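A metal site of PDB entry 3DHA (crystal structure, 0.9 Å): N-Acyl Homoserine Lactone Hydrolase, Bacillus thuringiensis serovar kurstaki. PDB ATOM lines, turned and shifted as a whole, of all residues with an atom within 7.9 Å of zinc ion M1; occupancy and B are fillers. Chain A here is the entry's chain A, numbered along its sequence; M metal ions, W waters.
ND1 of His 173 lies within hydrogen-bond range of O of Ala 210, 2.8 Å away. A ring nitrogen (ND1) of His 108 sits at hydrogen-bond distance from the side-chain hydroxyl (OG) of Ser 107 (2.9 Å). N of Asp 195 sits at hydrogen-bond distance from NE2 of His 177, 2.9 Å away. ND1 of His 113 is in hydrogen-bond range of OG of Ser 107, 3.4 Å away.
Zinc ion M1 is bound by water W1, NE2 of His 173, NE2 of His 108 and ND1 of His 110. Zinc ion M1 has four donor atoms within binding distance. Slightly farther from zinc ion M1 lies the side-chain carboxylate (OD2) of Asp 195 (2.6 Å).
NE2 of His 113 touches zinc ion M1, at 3.98 Å. Of the 21 residues printed, 5 come within 4 Å of zinc ion M1. Along chain A the residues within 4 Å of zinc ion M1 span positions 108 to 195.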
ATOM      1  N   LEU A  20     -32.514 -12.882 -33.922  1.00  0.00           N
ATOM      2  CA  LEU A  20     -33.259 -13.691 -33.009  1.00  0.00           C
ATOM      3  C   LEU A  20     -34.433 -12.821 -32.515  1.00  0.00           C
ATOM      4  O   LEU A  20     -34.293 -11.600 -32.393  1.00  0.00           O
ATOM      5  CB  LEU A  20     -32.434 -14.160 -31.821  1.00  0.00           C
ATOM      6  CG  LEU A  20     -31.786 -15.528 -31.824  1.00  0.00           C
ATOM      7  CD1 LEU A  20     -31.223 -15.965 -33.150  1.00  0.00           C
ATOM      8  CD2 LEU A  20     -30.685 -15.566 -30.741  1.00  0.00           C
ATOM      9  N   SER A 107     -16.894 -23.067 -27.666  1.00  0.00           N
ATOM     10  CA  SER A 107     -17.705 -22.858 -26.483  1.00  0.00           C
ATOM     11  C   SER A 107     -18.841 -23.838 -26.420  1.00  0.00           C
ATOM     12  O   SER A 107     -19.226 -24.349 -25.390  1.00  0.00           O
ATOM     13  CB  SER A 107     -18.231 -21.425 -26.428  1.00  0.00           C
ATOM     14  OG  SER A 107     -19.066 -21.163 -27.542  1.00  0.00           O
ATOM     15  N   HIS A 108     -19.453 -24.066 -27.613  1.00  0.00           N
ATOM     16  CA  HIS A 108     -20.525 -25.000 -27.825  1.00  0.00           C
ATOM     17  C   HIS A 108     -20.688 -25.135 -29.334  1.00  0.00           C
ATOM     18  O   HIS A 108     -20.009 -24.467 -30.080  1.00  0.00           O
ATOM     19  CB  HIS A 108     -21.791 -24.568 -27.077  1.00  0.00           C
ATOM     20  CG  HIS A 108     -22.422 -23.270 -27.466  1.00  0.00           C
ATOM     21  ND1 HIS A 108     -21.791 -22.039 -27.449  1.00  0.00           N
ATOM     22  CD2 HIS A 108     -23.715 -23.009 -27.760  1.00  0.00           C
ATOM     23  CE1 HIS A 108     -22.699 -21.092 -27.706  1.00  0.00           C
ATOM     24  NE2 HIS A 108     -23.892 -21.633 -27.931  1.00  0.00           N
ATOM     25  N   LEU A 109     -21.610 -26.015 -29.741  1.00  0.00           N
ATOM     26  CA  LEU A 109     -21.717 -26.414 -31.138  1.00  0.00           C
ATOM     27  C   LEU A 109     -22.954 -25.874 -31.808  1.00  0.00           C
ATOM     28  O   LEU A 109     -23.353 -26.347 -32.895  1.00  0.00           O
ATOM     29  CB  LEU A 109     -21.533 -27.932 -31.324  1.00  0.00           C
ATOM     30  CG  LEU A 109     -20.182 -28.469 -30.879  1.00  0.00           C
ATOM     31  CD1 LEU A 109     -20.176 -29.996 -31.004  1.00  0.00           C
ATOM     32  CD2 LEU A 109     -18.998 -27.893 -31.630  1.00  0.00           C
ATOM     33  N   HIS A 110     -23.555 -24.797 -31.250  1.00  0.00           N
ATOM     34  CA  HIS A 110     -24.567 -24.053 -31.998  1.00  0.00           C
ATOM     35  C   HIS A 110     -23.953 -23.511 -33.283  1.00  0.00           C
ATOM     36  O   HIS A 110     -22.728 -23.233 -33.359  1.00  0.00           O
ATOM     37  CB  HIS A 110     -25.132 -22.953 -31.119  1.00  0.00           C
ATOM     38  CG  HIS A 110     -26.088 -23.462 -30.065  1.00  0.00           C
ATOM     39  ND1 HIS A 110     -26.526 -22.641 -29.063  1.00  0.00           N
ATOM     40  CD2 HIS A 110     -26.625 -24.693 -29.910  1.00  0.00           C
ATOM     41  CE1 HIS A 110     -27.348 -23.374 -28.296  1.00  0.00           C
ATOM     42  NE2 HIS A 110     -27.425 -24.615 -28.771  1.00  0.00           N
ATOM     43  N   PHE A 111     -24.825 -23.231 -34.240  1.00  0.00           N
ATOM     44  CA  PHE A 111     -24.359 -22.880 -35.586  1.00  0.00           C
ATOM     45  C   PHE A 111     -23.562 -21.573 -35.673  1.00  0.00           C
ATOM     46  O   PHE A 111     -22.757 -21.400 -36.598  1.00  0.00           O
ATOM     47  CB  PHE A 111     -25.547 -22.870 -36.591  1.00  0.00           C
ATOM     48  CG  PHE A 111     -26.190 -21.523 -36.752  1.00  0.00           C
ATOM     49  CD1 PHE A 111     -26.036 -20.873 -37.945  1.00  0.00           C
ATOM     50  CD2 PHE A 111     -26.920 -20.878 -35.753  1.00  0.00           C
ATOM     51  CE1 PHE A 111     -26.560 -19.596 -38.187  1.00  0.00           C
ATOM     52  CE2 PHE A 111     -27.407 -19.551 -35.944  1.00  0.00           C
ATOM     53  CZ  PHE A 111     -27.191 -18.943 -37.157  1.00  0.00           C
ATOM     54  N   ASP A 112     -23.816 -20.664 -34.725  1.00  0.00           N
ATOM     55  CA  ASP A 112     -23.140 -19.372 -34.688  1.00  0.00           C
ATOM     56  C   ASP A 112     -21.815 -19.431 -33.976  1.00  0.00           C
ATOM     57  O   ASP A 112     -21.155 -18.403 -33.910  1.00  0.00           O
ATOM     58  CB  ASP A 112     -24.111 -18.313 -34.110  1.00  0.00           C
ATOM     59  CG  ASP A 112     -24.694 -18.642 -32.738  1.00  0.00           C
ATOM     60  OD1 ASP A 112     -24.720 -17.710 -31.895  1.00  0.00           O
ATOM     61  OD2 ASP A 112     -25.200 -19.761 -32.517  1.00  0.00           O
ATOM     62  N   HIS A 113     -21.414 -20.607 -33.489  1.00  0.00           N
ATOM     63  CA  HIS A 113     -20.173 -20.793 -32.758  1.00  0.00           C
ATOM     64  C   HIS A 113     -19.286 -21.832 -33.386  1.00  0.00           C
ATOM     65  O   HIS A 113     -18.054 -21.757 -33.186  1.00  0.00           O
ATOM     66  CB  HIS A 113     -20.455 -21.219 -31.308  1.00  0.00           C
ATOM     67  CG  HIS A 113     -21.205 -20.152 -30.613  1.00  0.00           C
ATOM     68  ND1 HIS A 113     -20.600 -19.188 -29.860  1.00  0.00           N
ATOM     69  CD2 HIS A 113     -22.479 -19.792 -30.607  1.00  0.00           C
ATOM     70  CE1 HIS A 113     -21.565 -18.305 -29.439  1.00  0.00           C
ATOM     71  NE2 HIS A 113     -22.751 -18.659 -29.890  1.00  0.00           N
ATOM     72  N   GLU A 131     -21.248 -31.710 -24.910  1.00  0.00           N
ATOM     73  CA  GLU A 131     -21.641 -30.970 -26.103  1.00  0.00           C
ATOM     74  C   GLU A 131     -21.475 -31.800 -27.368  1.00  0.00           C
ATOM     75  O   GLU A 131     -22.347 -31.843 -28.232  1.00  0.00           O
ATOM     76  CB  GLU A 131     -20.830 -29.686 -26.204  1.00  0.00           C
ATOM     77  CG  GLU A 131     -21.372 -28.768 -27.304  1.00  0.00           C
ATOM     78  CD  GLU A 131     -22.688 -28.082 -27.002  1.00  0.00           C
ATOM     79  OE1 GLU A 131     -23.154 -28.106 -25.819  1.00  0.00           O
ATOM     80  OE2 GLU A 131     -23.289 -27.509 -27.964  1.00  0.00           O
ATOM     81  N   TYR A 141     -28.962 -29.960 -33.907  1.00  0.00           N
ATOM     82  CA  TYR A 141     -27.655 -29.401 -34.320  1.00  0.00           C
ATOM     83  C   TYR A 141     -27.426 -29.544 -35.804  1.00  0.00           C
ATOM     84  O   TYR A 141     -27.786 -30.578 -36.400  1.00  0.00           O
ATOM     85  CB  TYR A 141     -26.571 -30.161 -33.551  1.00  0.00           C
ATOM     86  CG  TYR A 141     -26.366 -29.703 -32.120  1.00  0.00           C
ATOM     87  CD1 TYR A 141     -27.113 -30.221 -31.100  1.00  0.00           C
ATOM     88  CD2 TYR A 141     -25.417 -28.741 -31.790  1.00  0.00           C
ATOM     89  CE1 TYR A 141     -26.937 -29.791 -29.769  1.00  0.00           C
ATOM     90  CE2 TYR A 141     -25.228 -28.321 -30.501  1.00  0.00           C
ATOM     91  CZ  TYR A 141     -25.980 -28.847 -29.502  1.00  0.00           C
ATOM     92  OH  TYR A 141     -25.783 -28.462 -28.187  1.00  0.00           O
ATOM     93  N   HIS A 173     -27.379 -23.422 -21.346  1.00  0.00           N
ATOM     94  CA  HIS A 173     -27.788 -22.896 -22.657  1.00  0.00           C
ATOM     95  C   HIS A 173     -27.684 -23.983 -23.704  1.00  0.00           C
ATOM     96  O   HIS A 173     -28.514 -24.042 -24.615  1.00  0.00           O
ATOM     97  CB  HIS A 173     -26.897 -21.725 -22.999  1.00  0.00           C
ATOM     98  CG  HIS A 173     -27.039 -21.276 -24.428  1.00  0.00           C
ATOM     99  ND1 HIS A 173     -28.124 -20.593 -24.941  1.00  0.00           N
ATOM    100  CD2 HIS A 173     -26.188 -21.432 -25.458  1.00  0.00           C
ATOM    101  CE1 HIS A 173     -27.910 -20.358 -26.238  1.00  0.00           C
ATOM    102  NE2 HIS A 173     -26.713 -20.811 -26.617  1.00  0.00           N
ATOM    103  N   SER A 174     -26.640 -24.804 -23.613  1.00  0.00           N
ATOM    104  CA  SER A 174     -26.517 -26.037 -24.373  1.00  0.00           C
ATOM    105  C   SER A 174     -25.962 -27.112 -23.410  1.00  0.00           C
ATOM    106  O   SER A 174     -25.456 -26.773 -22.326  1.00  0.00           O
ATOM    107  CB  SER A 174     -25.625 -25.862 -25.581  1.00  0.00           C
ATOM    108  OG  SER A 174     -24.274 -25.671 -25.193  1.00  0.00           O
ATOM    109  N   HIS A 177     -22.061 -26.463 -22.737  1.00  0.00           N
ATOM    110  CA  HIS A 177     -21.546 -25.114 -22.919  1.00  0.00           C
ATOM    111  C   HIS A 177     -20.388 -24.879 -21.960  1.00  0.00           C
ATOM    112  O   HIS A 177     -20.423 -25.276 -20.779  1.00  0.00           O
ATOM    113  CB  HIS A 177     -22.708 -24.106 -22.698  1.00  0.00           C
ATOM    114  CG  HIS A 177     -22.242 -22.712 -22.931  1.00  0.00           C
ATOM    115  ND1 HIS A 177     -21.601 -21.953 -21.987  1.00  0.00           N
ATOM    116  CD2 HIS A 177     -22.309 -21.960 -24.079  1.00  0.00           C
ATOM    117  CE1 HIS A 177     -21.276 -20.796 -22.549  1.00  0.00           C
ATOM    118  NE2 HIS A 177     -21.709 -20.738 -23.818  1.00  0.00           N
ATOM    119  N   ILE A 194     -19.564 -16.171 -22.912  1.00  0.00           N
ATOM    120  CA  ILE A 194     -20.182 -16.745 -24.104  1.00  0.00           C
ATOM    121  C   ILE A 194     -21.677 -16.808 -23.828  1.00  0.00           C
ATOM    122  O   ILE A 194     -22.226 -15.822 -23.284  1.00  0.00           O
ATOM    123  CB  ILE A 194     -19.508 -18.031 -24.659  1.00  0.00           C
ATOM    124  CG1 ILE A 194     -18.000 -18.034 -24.437  1.00  0.00           C
ATOM    125  CG2 ILE A 194     -19.915 -18.242 -26.116  1.00  0.00           C
ATOM    126  CD1 ILE A 194     -17.226 -17.061 -25.298  1.00  0.00           C
ATOM    127  N   ASP A 195     -22.350 -17.888 -24.149  1.00  0.00           N
ATOM    128  CA  ASP A 195     -23.782 -17.910 -24.068  1.00  0.00           C
ATOM    129  C   ASP A 195     -24.313 -18.460 -22.763  1.00  0.00           C
ATOM    130  O   ASP A 195     -25.488 -18.782 -22.637  1.00  0.00           O
ATOM    131  CB  ASP A 195     -24.371 -18.704 -25.274  1.00  0.00           C
ATOM    132  CG  ASP A 195     -24.191 -17.939 -26.591  1.00  0.00           C
ATOM    133  OD1 ASP A 195     -23.578 -16.852 -26.656  1.00  0.00           O
ATOM    134  OD2 ASP A 195     -24.690 -18.508 -27.594  1.00  0.00           O
ATOM    135  N   ALA A 196     -23.465 -18.495 -21.731  1.00  0.00           N
ATOM    136  CA  ALA A 196     -23.926 -18.714 -20.385  1.00  0.00           C
ATOM    137  C   ALA A 196     -24.742 -17.493 -19.951  1.00  0.00           C
ATOM    138  O   ALA A 196     -25.425 -17.552 -18.969  1.00  0.00           O
ATOM    139  CB  ALA A 196     -22.796 -19.086 -19.445  1.00  0.00           C
ATOM    140  N   TYR A 198     -26.546 -14.341 -22.548  1.00  0.00           N
ATOM    141  CA  TYR A 198     -26.527 -13.531 -23.752  1.00  0.00           C
ATOM    142  C   TYR A 198     -26.265 -12.071 -23.440  1.00  0.00           C
ATOM    143  O   TYR A 198     -25.533 -11.404 -24.172  1.00  0.00           O
ATOM    144  CB  TYR A 198     -27.883 -13.577 -24.470  1.00  0.00           C
ATOM    145  CG  TYR A 198     -28.187 -14.791 -25.300  1.00  0.00           C
ATOM    146  CD1 TYR A 198     -27.357 -15.830 -25.578  1.00  0.00           C
ATOM    147  CD2 TYR A 198     -29.426 -14.861 -25.872  1.00  0.00           C
ATOM    148  CE1 TYR A 198     -27.707 -16.934 -26.383  1.00  0.00           C
ATOM    149  CE2 TYR A 198     -29.785 -15.901 -26.680  1.00  0.00           C
ATOM    150  CZ  TYR A 198     -28.974 -16.936 -26.956  1.00  0.00           C
ATOM    151  OH  TYR A 198     -29.399 -17.943 -27.764  1.00  0.00           O
ATOM    152  N   PHE A 209     -33.402 -16.825 -20.721  1.00  0.00           N
ATOM    153  CA  PHE A 209     -33.051 -16.622 -22.097  1.00  0.00           C
ATOM    154  C   PHE A 209     -32.980 -17.973 -22.770  1.00  0.00           C
ATOM    155  O   PHE A 209     -33.115 -19.011 -22.109  1.00  0.00           O
ATOM    156  CB  PHE A 209     -31.757 -15.859 -22.289  1.00  0.00           C
ATOM    157  CG  PHE A 209     -30.556 -16.575 -21.782  1.00  0.00           C
ATOM    158  CD1 PHE A 209     -29.642 -17.193 -22.668  1.00  0.00           C
ATOM    159  CD2 PHE A 209     -30.262 -16.622 -20.415  1.00  0.00           C
ATOM    160  CE1 PHE A 209     -28.520 -17.808 -22.214  1.00  0.00           C
ATOM    161  CE2 PHE A 209     -29.111 -17.293 -19.969  1.00  0.00           C
ATOM    162  CZ  PHE A 209     -28.264 -17.836 -20.852  1.00  0.00           C
ATOM    163  N   ALA A 210     -32.843 -18.006 -24.102  1.00  0.00           N
ATOM    164  CA  ALA A 210     -32.977 -19.226 -24.882  1.00  0.00           C
ATOM    165  C   ALA A 210     -31.938 -20.246 -24.383  1.00  0.00           C
ATOM    166  O   ALA A 210     -30.765 -19.853 -24.169  1.00  0.00           O
ATOM    167  CB  ALA A 210     -32.760 -18.880 -26.321  1.00  0.00           C
ATOM    168  N   GLY A 211     -32.351 -21.471 -24.232  1.00  0.00           N
ATOM    169  CA  GLY A 211     -31.379 -22.495 -23.928  1.00  0.00           C
ATOM    170  C   GLY A 211     -32.069 -23.799 -23.732  1.00  0.00           C
ATOM    171  O   GLY A 211     -33.289 -23.940 -23.585  1.00  0.00           O
ATOM    172  N   HIS A 239     -24.161 -12.174 -26.509  1.00  0.00           N
ATOM    173  CA  HIS A 239     -24.934 -11.586 -27.632  1.00  0.00           C
ATOM    174  C   HIS A 239     -25.661 -10.366 -27.148  1.00  0.00           C
ATOM    175  O   HIS A 239     -26.897 -10.371 -27.007  1.00  0.00           O
ATOM    176  CB  HIS A 239     -25.890 -12.633 -28.201  1.00  0.00           C
ATOM    177  CG  HIS A 239     -25.349 -13.845 -28.865  1.00  0.00           C
ATOM    178  ND1 HIS A 239     -24.641 -13.828 -30.066  1.00  0.00           N
ATOM    179  CD2 HIS A 239     -25.468 -15.150 -28.542  1.00  0.00           C
ATOM    180  CE1 HIS A 239     -24.370 -15.079 -30.379  1.00  0.00           C
ATOM    181  NE2 HIS A 239     -24.853 -15.950 -29.481  1.00  0.00           N
HETATM  182 ZN    ZN M   1     -25.708 -20.820 -28.339  1.00  0.00          ZN
HETATM  183 ZN    ZN M   2     -24.601 -17.927 -29.574  1.00  0.00          ZN
HETATM  184  O   HOH W   1     -25.862 -19.490 -29.750  1.00  0.00           O
